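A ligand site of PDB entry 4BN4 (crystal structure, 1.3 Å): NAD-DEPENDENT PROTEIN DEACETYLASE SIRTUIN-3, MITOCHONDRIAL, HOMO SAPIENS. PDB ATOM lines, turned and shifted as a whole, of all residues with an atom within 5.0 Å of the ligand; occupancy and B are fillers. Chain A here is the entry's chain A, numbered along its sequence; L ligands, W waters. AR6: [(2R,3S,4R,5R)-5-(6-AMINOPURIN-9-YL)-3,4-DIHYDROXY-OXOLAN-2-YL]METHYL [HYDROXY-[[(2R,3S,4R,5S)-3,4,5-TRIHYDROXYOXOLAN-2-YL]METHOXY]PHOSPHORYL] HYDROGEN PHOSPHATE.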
ATOM      1  N   GLY A  30     -14.324   7.588   8.607  1.00  0.00           N
ATOM      2  CA  GLY A  30     -13.925   6.199   8.271  1.00  0.00           C
ATOM      3  C   GLY A  30     -12.465   5.987   8.466  1.00  0.00           C
ATOM      4  O   GLY A  30     -11.793   6.676   9.208  1.00  0.00           O
ATOM      5  N   ALA A  31     -12.068   4.902   7.825  1.00  0.00           N
ATOM      6  CA  ALA A  31     -10.763   4.316   8.176  1.00  0.00           C
ATOM      7  C   ALA A  31      -9.532   5.166   7.822  1.00  0.00           C
ATOM      8  O   ALA A  31      -8.458   5.016   8.372  1.00  0.00           O
ATOM      9  CB  ALA A  31     -10.700   2.930   7.473  1.00  0.00           C
ATOM     10  N   GLY A  32      -9.748   6.111   6.917  1.00  0.00           N
ATOM     11  CA  GLY A  32      -8.702   7.048   6.626  1.00  0.00           C
ATOM     12  C   GLY A  32      -8.290   7.869   7.819  1.00  0.00           C
ATOM     13  O   GLY A  32      -7.121   8.329   7.848  1.00  0.00           O
ATOM     14  N   THR A  35      -5.283   5.921   9.600  1.00  0.00           N
ATOM     15  CA  THR A  35      -3.994   5.659   8.979  1.00  0.00           C
ATOM     16  C   THR A  35      -2.851   6.471   9.621  1.00  0.00           C
ATOM     17  O   THR A  35      -1.743   5.946   9.772  1.00  0.00           O
ATOM     18  CB  THR A  35      -4.067   5.754   7.494  1.00  0.00           C
ATOM     19  OG1 THR A  35      -4.362   7.121   7.054  1.00  0.00           O
ATOM     20  CG2 THR A  35      -5.063   4.767   6.847  1.00  0.00           C
ATOM     21  N   PRO A  36      -3.092   7.737  10.086  1.00  0.00           N
ATOM     22  CA  PRO A  36      -1.992   8.404  10.731  1.00  0.00           C
ATOM     23  C   PRO A  36      -1.653   7.809  12.119  1.00  0.00           C
ATOM     24  O   PRO A  36      -0.607   8.115  12.641  1.00  0.00           O
ATOM     25  CB  PRO A  36      -2.466   9.857  10.857  1.00  0.00           C
ATOM     26  CG  PRO A  36      -3.581   9.972   9.898  1.00  0.00           C
ATOM     27  CD  PRO A  36      -4.245   8.619   9.867  1.00  0.00           C
ATOM     28  N   ASP A  41      -6.302   1.385   6.157  1.00  0.00           N
ATOM     29  CA  ASP A  41      -7.668   1.429   5.787  1.00  0.00           C
ATOM     30  C   ASP A  41      -8.077   0.157   5.023  1.00  0.00           C
ATOM     31  O   ASP A  41      -7.332  -0.831   5.084  1.00  0.00           O
ATOM     32  CB  ASP A  41      -7.987   2.725   4.985  1.00  0.00           C
ATOM     33  CG  ASP A  41      -7.366   2.780   3.568  1.00  0.00           C
ATOM     34  OD1 ASP A  41      -6.890   1.713   3.062  1.00  0.00           O
ATOM     35  OD2 ASP A  41      -7.440   3.920   2.994  1.00  0.00           O
ATOM     36  N   PHE A  42      -9.288   0.183   4.450  1.00  0.00           N
ATOM     37  CA  PHE A  42      -9.812  -1.000   3.742  1.00  0.00           C
ATOM     38  C   PHE A  42      -9.443  -0.997   2.259  1.00  0.00           C
ATOM     39  O   PHE A  42      -9.033  -2.038   1.716  1.00  0.00           O
ATOM     40  CB  PHE A  42     -11.305  -1.124   3.895  1.00  0.00           C
ATOM     41  CG  PHE A  42     -11.722  -1.452   5.276  1.00  0.00           C
ATOM     42  CD1 PHE A  42     -11.582  -2.750   5.731  1.00  0.00           C
ATOM     43  CD2 PHE A  42     -12.166  -0.492   6.151  1.00  0.00           C
ATOM     44  CE1 PHE A  42     -11.923  -3.072   7.024  1.00  0.00           C
ATOM     45  CE2 PHE A  42     -12.536  -0.818   7.457  1.00  0.00           C
ATOM     46  CZ  PHE A  42     -12.361  -2.097   7.927  1.00  0.00           C
ATOM     47  N   ARG A  43      -9.576   0.152   1.589  1.00  0.00           N
ATOM     48  CA  ARG A  43      -9.626   0.168   0.151  1.00  0.00           C
ATOM     49  C   ARG A  43      -8.491   0.924  -0.552  1.00  0.00           C
ATOM     50  O   ARG A  43      -8.466   0.904  -1.796  1.00  0.00           O
ATOM     51  CB  ARG A  43     -10.976   0.719  -0.315  1.00  0.00           C
ATOM     52  CG  ARG A  43     -12.165  -0.170   0.011  1.00  0.00           C
ATOM     53  CD  ARG A  43     -13.507   0.336  -0.499  1.00  0.00           C
ATOM     54  NE  ARG A  43     -14.565  -0.590  -0.111  1.00  0.00           N
ATOM     55  CZ  ARG A  43     -15.082  -0.652   1.105  1.00  0.00           C
ATOM     56  NH1 ARG A  43     -15.950  -1.597   1.370  1.00  0.00           N
ATOM     57  NH2 ARG A  43     -14.763   0.255   2.042  1.00  0.00           N
ATOM     58  N   SER A  44      -7.512   1.474   0.146  1.00  0.00           N
ATOM     59  CA  SER A  44      -6.367   2.095  -0.550  1.00  0.00           C
ATOM     60  C   SER A  44      -5.615   0.971  -1.296  1.00  0.00           C
ATOM     61  O   SER A  44      -5.344  -0.114  -0.732  1.00  0.00           O
ATOM     62  CB  SER A  44      -5.420   2.766   0.354  1.00  0.00           C
ATOM     63  OG  SER A  44      -5.996   3.939   0.821  1.00  0.00           O
ATOM     64  N   TYR A  50      -8.240  -4.839   2.356  1.00  0.00           N
ATOM     65  CA  TYR A  50      -8.874  -5.701   1.357  1.00  0.00           C
ATOM     66  C   TYR A  50      -7.975  -6.101   0.208  1.00  0.00           C
ATOM     67  O   TYR A  50      -8.177  -7.172  -0.368  1.00  0.00           O
ATOM     68  CB  TYR A  50     -10.196  -5.081   0.900  1.00  0.00           C
ATOM     69  CG  TYR A  50     -11.344  -5.033   1.928  1.00  0.00           C
ATOM     70  CD1 TYR A  50     -11.368  -5.839   3.065  1.00  0.00           C
ATOM     71  CD2 TYR A  50     -12.475  -4.245   1.699  1.00  0.00           C
ATOM     72  CE1 TYR A  50     -12.477  -5.869   3.899  1.00  0.00           C
ATOM     73  CE2 TYR A  50     -13.526  -4.245   2.557  1.00  0.00           C
ATOM     74  CZ  TYR A  50     -13.525  -5.096   3.632  1.00  0.00           C
ATOM     75  OH  TYR A  50     -14.571  -5.117   4.526  1.00  0.00           O
ATOM     76  N   PHE A  65     -15.853 -10.299   7.551  1.00  0.00           N
ATOM     77  CA  PHE A  65     -17.016  -9.804   8.246  1.00  0.00           C
ATOM     78  C   PHE A  65     -18.335 -10.441   7.780  1.00  0.00           C
ATOM     79  O   PHE A  65     -19.397  -9.835   7.885  1.00  0.00           O
ATOM     80  CB  PHE A  65     -17.169  -8.270   8.094  1.00  0.00           C
ATOM     81  CG  PHE A  65     -15.955  -7.485   8.477  1.00  0.00           C
ATOM     82  CD1 PHE A  65     -15.397  -7.575   9.717  1.00  0.00           C
ATOM     83  CD2 PHE A  65     -15.340  -6.621   7.571  1.00  0.00           C
ATOM     84  CE1 PHE A  65     -14.255  -6.863  10.080  1.00  0.00           C
ATOM     85  CE2 PHE A  65     -14.206  -5.901   7.942  1.00  0.00           C
ATOM     86  CZ  PHE A  65     -13.704  -5.958   9.193  1.00  0.00           C
ATOM     87  N   GLN A 113     -17.560   4.661  11.258  1.00  0.00           N
ATOM     88  CA  GLN A 113     -17.562   3.346  10.660  1.00  0.00           C
ATOM     89  C   GLN A 113     -16.433   2.460  11.186  1.00  0.00           C
ATOM     90  O   GLN A 113     -16.368   1.290  10.876  1.00  0.00           O
ATOM     91  CB  GLN A 113     -17.418   3.451   9.133  1.00  0.00           C
ATOM     92  CG  GLN A 113     -18.577   4.159   8.478  1.00  0.00           C
ATOM     93  CD  GLN A 113     -18.284   4.552   7.063  1.00  0.00           C
ATOM     94  OE1 GLN A 113     -18.791   3.965   6.123  1.00  0.00           O
ATOM     95  NE2 GLN A 113     -17.511   5.551   6.918  1.00  0.00           N
ATOM     96  N   ASN A 114     -15.459   3.060  11.892  1.00  0.00           N
ATOM     97  CA  ASN A 114     -14.266   2.366  12.346  1.00  0.00           C
ATOM     98  C   ASN A 114     -14.606   1.452  13.537  1.00  0.00           C
ATOM     99  O   ASN A 114     -15.517   1.737  14.308  1.00  0.00           O
ATOM    100  CB  ASN A 114     -13.156   3.330  12.748  1.00  0.00           C
ATOM    101  CG  ASN A 114     -12.665   4.183  11.578  1.00  0.00           C
ATOM    102  OD1 ASN A 114     -11.908   5.208  11.867  1.00  0.00           O
ATOM    103  ND2 ASN A 114     -12.975   3.830  10.439  1.00  0.00           N
ATOM    104  N   HIS A 133     -20.579   0.669  13.223  1.00  0.00           N
ATOM    105  CA  HIS A 133     -20.214  -0.676  12.850  1.00  0.00           C
ATOM    106  C   HIS A 133     -19.796  -1.580  14.040  1.00  0.00           C
ATOM    107  O   HIS A 133     -19.217  -2.674  13.875  1.00  0.00           O
ATOM    108  CB  HIS A 133     -19.132  -0.676  11.835  1.00  0.00           C
ATOM    109  CG  HIS A 133     -19.606  -0.298  10.475  1.00  0.00           C
ATOM    110  ND1 HIS A 133     -18.772  -0.081   9.404  1.00  0.00           N
ATOM    111  CD2 HIS A 133     -20.861  -0.067  10.009  1.00  0.00           C
ATOM    112  CE1 HIS A 133     -19.487   0.255   8.350  1.00  0.00           C
ATOM    113  NE2 HIS A 133     -20.763   0.238   8.683  1.00  0.00           N
ATOM    114  N   PHE A 179     -21.864  -8.445   7.829  1.00  0.00           N
ATOM    115  CA  PHE A 179     -22.820  -8.270   6.715  1.00  0.00           C
ATOM    116  C   PHE A 179     -24.119  -8.966   7.017  1.00  0.00           C
ATOM    117  O   PHE A 179     -24.174 -10.069   7.543  1.00  0.00           O
ATOM    118  CB  PHE A 179     -22.236  -8.812   5.420  1.00  0.00           C
ATOM    119  CG  PHE A 179     -21.105  -7.981   4.875  1.00  0.00           C
ATOM    120  CD1 PHE A 179     -21.396  -6.754   4.198  1.00  0.00           C
ATOM    121  CD2 PHE A 179     -19.760  -8.310   5.109  1.00  0.00           C
ATOM    122  CE1 PHE A 179     -20.362  -5.971   3.702  1.00  0.00           C
ATOM    123  CE2 PHE A 179     -18.722  -7.512   4.626  1.00  0.00           C
ATOM    124  CZ  PHE A 179     -19.028  -6.343   3.895  1.00  0.00           C
ATOM    125  N   GLY A 204     -11.952  11.073   5.893  1.00  0.00           N
ATOM    126  CA  GLY A 204     -11.299   9.760   5.730  1.00  0.00           C
ATOM    127  C   GLY A 204     -12.243   8.587   5.486  1.00  0.00           C
ATOM    128  O   GLY A 204     -12.065   7.510   6.096  1.00  0.00           O
ATOM    129  N   THR A 205     -13.171   8.729   4.533  1.00  0.00           N
ATOM    130  CA  THR A 205     -14.063   7.649   4.148  1.00  0.00           C
ATOM    131  C   THR A 205     -14.224   7.714   2.644  1.00  0.00           C
ATOM    132  O   THR A 205     -14.261   8.802   2.071  1.00  0.00           O
ATOM    133  CB  THR A 205     -15.370   7.639   4.897  1.00  0.00           C
ATOM    134  OG1 THR A 205     -16.240   6.610   4.392  1.00  0.00           O
ATOM    135  CG2 THR A 205     -16.057   8.929   4.901  1.00  0.00           C
ATOM    136  N   SER A 206     -14.304   6.526   2.009  1.00  0.00           N
ATOM    137  CA  SER A 206     -14.565   6.446   0.584  1.00  0.00           C
ATOM    138  C   SER A 206     -16.012   6.567   0.229  1.00  0.00           C
ATOM    139  O   SER A 206     -16.352   6.727  -0.968  1.00  0.00           O
ATOM    140  CB  SER A 206     -14.031   5.119   0.070  1.00  0.00           C
ATOM    141  OG  SER A 206     -14.754   4.065   0.661  1.00  0.00           O
ATOM    142  N   LEU A 207     -16.940   6.596   1.186  1.00  0.00           N
ATOM    143  CA  LEU A 207     -18.361   6.634   0.956  1.00  0.00           C
ATOM    144  C   LEU A 207     -18.851   5.610  -0.077  1.00  0.00           C
ATOM    145  O   LEU A 207     -19.734   5.888  -0.860  1.00  0.00           O
ATOM    146  CB  LEU A 207     -18.770   8.069   0.580  1.00  0.00           C
ATOM    147  CG  LEU A 207     -18.490   9.152   1.609  1.00  0.00           C
ATOM    148  CD1 LEU A 207     -18.953  10.510   1.094  1.00  0.00           C
ATOM    149  CD2 LEU A 207     -19.152   8.814   2.936  1.00  0.00           C
ATOM    150  N   VAL A 209     -19.967   2.562   0.949  1.00  0.00           N
ATOM    151  CA  VAL A 209     -20.782   1.626   1.750  1.00  0.00           C
ATOM    152  C   VAL A 209     -21.933   2.415   2.325  1.00  0.00           C
ATOM    153  O   VAL A 209     -21.751   3.550   2.868  1.00  0.00           O
ATOM    154  CB  VAL A 209     -19.936   0.950   2.891  1.00  0.00           C
ATOM    155  CG1 VAL A 209     -20.731   0.021   3.738  1.00  0.00           C
ATOM    156  CG2 VAL A 209     -18.799   0.209   2.225  1.00  0.00           C
ATOM    157  N   ASN A 229     -10.296  14.479   2.843  1.00  0.00           N
ATOM    158  CA  ASN A 229     -10.039  13.118   2.340  1.00  0.00           C
ATOM    159  C   ASN A 229      -9.017  13.170   1.256  1.00  0.00           C
ATOM    160  O   ASN A 229      -8.891  14.214   0.594  1.00  0.00           O
ATOM    161  CB  ASN A 229     -11.350  12.494   1.858  1.00  0.00           C
ATOM    162  CG  ASN A 229     -11.280  10.996   1.774  1.00  0.00           C
ATOM    163  OD1 ASN A 229     -10.951  10.377   2.747  1.00  0.00           O
ATOM    164  ND2 ASN A 229     -11.614  10.396   0.620  1.00  0.00           N
ATOM    165  N   ARG A 230      -8.400  12.061   0.918  1.00  0.00           N
ATOM    166  CA  ARG A 230      -7.459  12.012  -0.229  1.00  0.00           C
ATOM    167  C   ARG A 230      -8.149  12.410  -1.547  1.00  0.00           C
ATOM    168  O   ARG A 230      -7.622  13.191  -2.342  1.00  0.00           O
ATOM    169  CB  ARG A 230      -6.850  10.613  -0.317  1.00  0.00           C
ATOM    170  CG  ARG A 230      -5.879  10.306  -1.452  1.00  0.00           C
ATOM    171  CD  ARG A 230      -5.153   9.001  -1.082  1.00  0.00           C
ATOM    172  NE  ARG A 230      -4.324   9.137   0.140  1.00  0.00           N
ATOM    173  CZ  ARG A 230      -3.976   8.144   0.954  1.00  0.00           C
ATOM    174  NH1 ARG A 230      -4.369   6.914   0.734  1.00  0.00           N
ATOM    175  NH2 ARG A 230      -3.217   8.365   1.987  1.00  0.00           N
ATOM    176  N   ASP A 231      -9.338  11.861  -1.744  1.00  0.00           N
ATOM    177  CA  ASP A 231     -10.142  11.966  -2.944  1.00  0.00           C
ATOM    178  C   ASP A 231     -11.549  12.482  -2.735  1.00  0.00           C
ATOM    179  O   ASP A 231     -12.156  12.324  -1.672  1.00  0.00           O
ATOM    180  CB  ASP A 231     -10.305  10.544  -3.531  1.00  0.00           C
ATOM    181  CG  ASP A 231      -8.980   9.855  -3.830  1.00  0.00           C
ATOM    182  OD1 ASP A 231      -8.059  10.504  -4.375  1.00  0.00           O
ATOM    183  OD2 ASP A 231      -8.907   8.636  -3.543  1.00  0.00           O
ATOM    184  N   VAL A 233     -15.255  11.995  -3.188  1.00  0.00           N
ATOM    185  CA  VAL A 233     -15.955  10.710  -3.175  1.00  0.00           C
ATOM    186  C   VAL A 233     -17.441  10.828  -2.983  1.00  0.00           C
ATOM    187  O   VAL A 233     -17.966  11.766  -2.359  1.00  0.00           O
ATOM    188  CB  VAL A 233     -15.402   9.814  -2.077  1.00  0.00           C
ATOM    189  CG1 VAL A 233     -14.012   9.367  -2.413  1.00  0.00           C
ATOM    190  CG2 VAL A 233     -15.375  10.514  -0.765  1.00  0.00           C
ATOM    191  N   GLY A 249      -6.414  15.832   0.054  1.00  0.00           N
ATOM    192  CA  GLY A 249      -5.001  15.536   0.411  1.00  0.00           C
ATOM    193  C   GLY A 249      -4.952  14.772   1.750  1.00  0.00           C
ATOM    194  O   GLY A 249      -5.987  14.242   2.186  1.00  0.00           O
ATOM    195  N   ASP A 250      -3.800  14.788   2.369  1.00  0.00           N
ATOM    196  CA  ASP A 250      -3.593  14.065   3.605  1.00  0.00           C
ATOM    197  C   ASP A 250      -4.546  14.603   4.683  1.00  0.00           C
ATOM    198  O   ASP A 250      -4.645  15.801   4.855  1.00  0.00           O
ATOM    199  CB  ASP A 250      -2.156  14.133   4.090  1.00  0.00           C
ATOM    200  CG  ASP A 250      -1.995  13.395   5.413  1.00  0.00           C
ATOM    201  OD1 ASP A 250      -2.015  12.162   5.430  1.00  0.00           O
ATOM    202  OD2 ASP A 250      -1.898  14.040   6.482  1.00  0.00           O
ATOM    203  N   VAL A 251      -5.137  13.729   5.505  1.00  0.00           N
ATOM    204  CA  VAL A 251      -6.127  14.117   6.456  1.00  0.00           C
ATOM    205  C   VAL A 251      -5.502  14.920   7.594  1.00  0.00           C
ATOM    206  O   VAL A 251      -6.112  15.834   8.106  1.00  0.00           O
ATOM    207  CB  VAL A 251      -6.912  12.881   6.960  1.00  0.00           C
ATOM    208  CG1 VAL A 251      -6.087  11.912   7.747  1.00  0.00           C
ATOM    209  CG2 VAL A 251      -8.198  13.328   7.621  1.00  0.00           C
HETATM  210  N1  AR6 L   1      -5.304  11.064   4.335  1.00  0.00           N
HETATM  211  C2  AR6 L   1      -6.435  11.272   3.622  1.00  0.00           C
HETATM  212  N3  AR6 L   1      -7.286  10.354   3.112  1.00  0.00           N
HETATM  213  C4  AR6 L   1      -6.963   9.081   3.445  1.00  0.00           C
HETATM  214  C5  AR6 L   1      -5.791   8.780   4.201  1.00  0.00           C
HETATM  215  C6  AR6 L   1      -4.994   9.807   4.699  1.00  0.00           C
HETATM  216  N6  AR6 L   1      -3.876   9.686   5.413  1.00  0.00           N
HETATM  217  N7  AR6 L   1      -5.772   7.412   4.320  1.00  0.00           N
HETATM  218  C8  AR6 L   1      -6.791   6.937   3.643  1.00  0.00           C
HETATM  219  N9  AR6 L   1      -7.563   7.964   3.104  1.00  0.00           N
HETATM  220  PA  AR6 L   1     -12.072   2.924   2.999  1.00  0.00           P
HETATM  221  PB  AR6 L   1     -14.222   3.332   4.923  1.00  0.00           P
HETATM  222  C1' AR6 L   1      -8.820   7.869   2.405  1.00  0.00           C
HETATM  223  O1A AR6 L   1     -13.106   2.441   1.980  1.00  0.00           O
HETATM  224  O1B AR6 L   1     -14.153   3.620   6.376  1.00  0.00           O
HETATM  225  C1D AR6 L   1     -15.670  -1.742   5.069  1.00  0.00           C
HETATM  226  O1D AR6 L   1     -16.274  -2.902   4.464  1.00  0.00           O
HETATM  227  C2' AR6 L   1      -8.858   6.856   1.278  1.00  0.00           C
HETATM  228  O2' AR6 L   1      -8.337   7.472   0.097  1.00  0.00           O
HETATM  229  O2A AR6 L   1     -10.754   2.289   3.119  1.00  0.00           O
HETATM  230  O2B AR6 L   1     -14.789   4.389   3.999  1.00  0.00           O
HETATM  231  C2D AR6 L   1     -15.879  -1.609   6.527  1.00  0.00           C
HETATM  232  O2D AR6 L   1     -17.171  -2.077   6.926  1.00  0.00           O
HETATM  233  C3' AR6 L   1     -10.301   6.509   1.207  1.00  0.00           C
HETATM  234  O3' AR6 L   1     -11.116   7.435   0.433  1.00  0.00           O
HETATM  235  O3A AR6 L   1     -12.789   2.949   4.463  1.00  0.00           O
HETATM  236  C3D AR6 L   1     -15.778  -0.110   6.650  1.00  0.00           C
HETATM  237  O3D AR6 L   1     -16.337   0.421   7.862  1.00  0.00           O
HETATM  238  C4' AR6 L   1     -10.744   6.598   2.689  1.00  0.00           C
HETATM  239  O4' AR6 L   1      -9.727   7.307   3.357  1.00  0.00           O
HETATM  240  C4D AR6 L   1     -16.570   0.363   5.459  1.00  0.00           C
HETATM  241  O4D AR6 L   1     -16.194  -0.559   4.474  1.00  0.00           O
HETATM  242  C5' AR6 L   1     -10.783   5.220   3.309  1.00  0.00           C
HETATM  243  O5' AR6 L   1     -11.846   4.450   2.644  1.00  0.00           O
HETATM  244  C5D AR6 L   1     -16.303   1.770   4.996  1.00  0.00           C
HETATM  245  O5D AR6 L   1     -14.924   1.906   4.670  1.00  0.00           O
HETATM  246  O   HOH W   1     -14.192   2.055   8.568  1.00  0.00           O
HETATM  247  O   HOH W   2      -6.782   5.584  -1.076  1.00  0.00           O
HETATM  248  O   HOH W   3      -3.536   5.030   3.459  1.00  0.00           O
HETATM  249  O   HOH W   4     -18.788  -3.020   4.144  1.00  0.00           O
HETATM  250  O   HOH W   5     -17.143   3.532   2.237  1.00  0.00           O
HETATM  251  O   HOH W   6     -10.860   7.010  -2.241  1.00  0.00           O
HETATM  252  O   HOH W   7     -14.423  -0.732  10.356  1.00  0.00           O
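The backbone NH of Thr 205 sits at hydrogen-bond distance from the side-chain amide oxygen of Asn 229 (3.3 Å).
OD1 of Asp 41 sits at hydrogen-bond distance from N of Arg 43 (3.4 Å).
The backbone NH (N) of Ala 31 sits at hydrogen-bond distance from the backbone carbonyl oxygen (O) of Gly 204 (3.1 Å).
N of Arg 230 is in hydrogen-bond range of O of Gly 249 (3.5 Å).
The side-chain amide oxygen (OD1) of Asn 229 sits close to the backbone NH (N) of Gly 204.
The backbone carbonyl oxygen (O) of Asp 231 sits at hydrogen-bond distance from the side-chain amide nitrogen (ND2) of Asn 229 (3.0 Å).
The backbone carbonyl oxygen (O) of Gly 32 lies within hydrogen-bond range of the side-chain hydroxyl (OG1) of Thr 35, at 3.1 Å.
O of Gly 204 lies close to N of Gly 30 (3.4 Å).
Water W1 lies within hydrogen-bond range of O1B of the ligand, ND2 of Asn 114 and O of Gln 113.
Water W2 lies within hydrogen-bond range of OG of Ser 44 (2.6 Å), O2' of the ligand (2.7 Å) and NH1 of Arg 230 (3.3 Å).
Water W6 bridges O3' of the ligand and OD2 of Asp 231.
Water W5 lies within hydrogen-bond range of OG of Ser 206, O2B of the ligand, N of Leu 207 and N of Val 209.
Water W7 lies within hydrogen-bond range of the backbone carbonyl oxygen (O) of Gln 113 (2.9 Å) and an oxygen (O3D) of the ligand (3.3 Å).
Water W3 lies within hydrogen-bond range of a nitrogen (N7) of the ligand (3.4 Å) and the guanidinium group (NH1) of Arg 230 (3.4 Å).
Gly 30 touches the ligand (CA to O1B, 3.2 Å).
Gly 32 touches the ligand (CA to O4', 3.4 Å).
Asp 41 touches the ligand (OD2 to C8, 3.2 Å).
Gly 204 touches the ligand (C to O4', 3.5 Å).
Val 209 touches the ligand (CG2 to O4D, 3.5 Å).
Asp 231 touches the ligand (OD2 to O2', 3.9 Å).
Gly 249 touches the ligand (O to C2, 3.3 Å).
Hydrophobic or aromatic side chains within 4 Å of the ligand: Ala 31, Phe 42, Tyr 50, His 133, Val 209 and Val 251.
The nearest printed residue that does not touch the ligand is Ser 44 (4.1 Å).
N of Ser 206 is in hydrogen-bond range of O2B of the ligand, 3.0 Å away.
The side-chain hydroxyl (OG) of Ser 206 lies within hydrogen-bond range of an oxygen (O1A) of the ligand (2.7 Å).
OG1 of Thr 205 lies within hydrogen-bond range of O2B of the ligand (2.7 Å).
The backbone NH of Arg 43 lies within hydrogen-bond range of an oxygen (O2A) of the ligand, at 2.9 Å.
The guanidinium group of Arg 43 lies within salt-bridge range of an oxygen (O1A) of the ligand, 2.7 Å away.
The side-chain hydroxyl of Tyr 50 lies within hydrogen-bond range of an oxygen (O1D) of the ligand (2.8 Å).
The backbone NH (N) of Ala 31 lies within hydrogen-bond range of an oxygen (O1B) of the ligand, at 2.8 Å.
N of Phe 42 is in hydrogen-bond range of O2A of the ligand, 2.9 Å away.
The backbone NH (N) of Val 251 sits at hydrogen-bond distance from a nitrogen (N1) of the ligand.
ND1 of His 133 lies within hydrogen-bond range of O3D of the ligand (2.9 Å).
N of Arg 230 sits at hydrogen-bond distance from N3 of the ligand.
An oxygen (O3') of the ligand is in hydrogen-bond range of the side-chain amide nitrogen (ND2) of Asn 229 (3.0 Å).
The side-chain hydroxyl of Thr 35 sits at hydrogen-bond distance from a nitrogen (N6) of the ligand (3.1 Å).
The side-chain carboxylate of Asp 250 lies within hydrogen-bond range of a nitrogen (N6) of the ligand, at 3.1 Å.
The backbone carbonyl oxygen (O) of Gln 113 is in hydrogen-bond range of an oxygen (O3D) of the ligand, at 3.1 Å.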
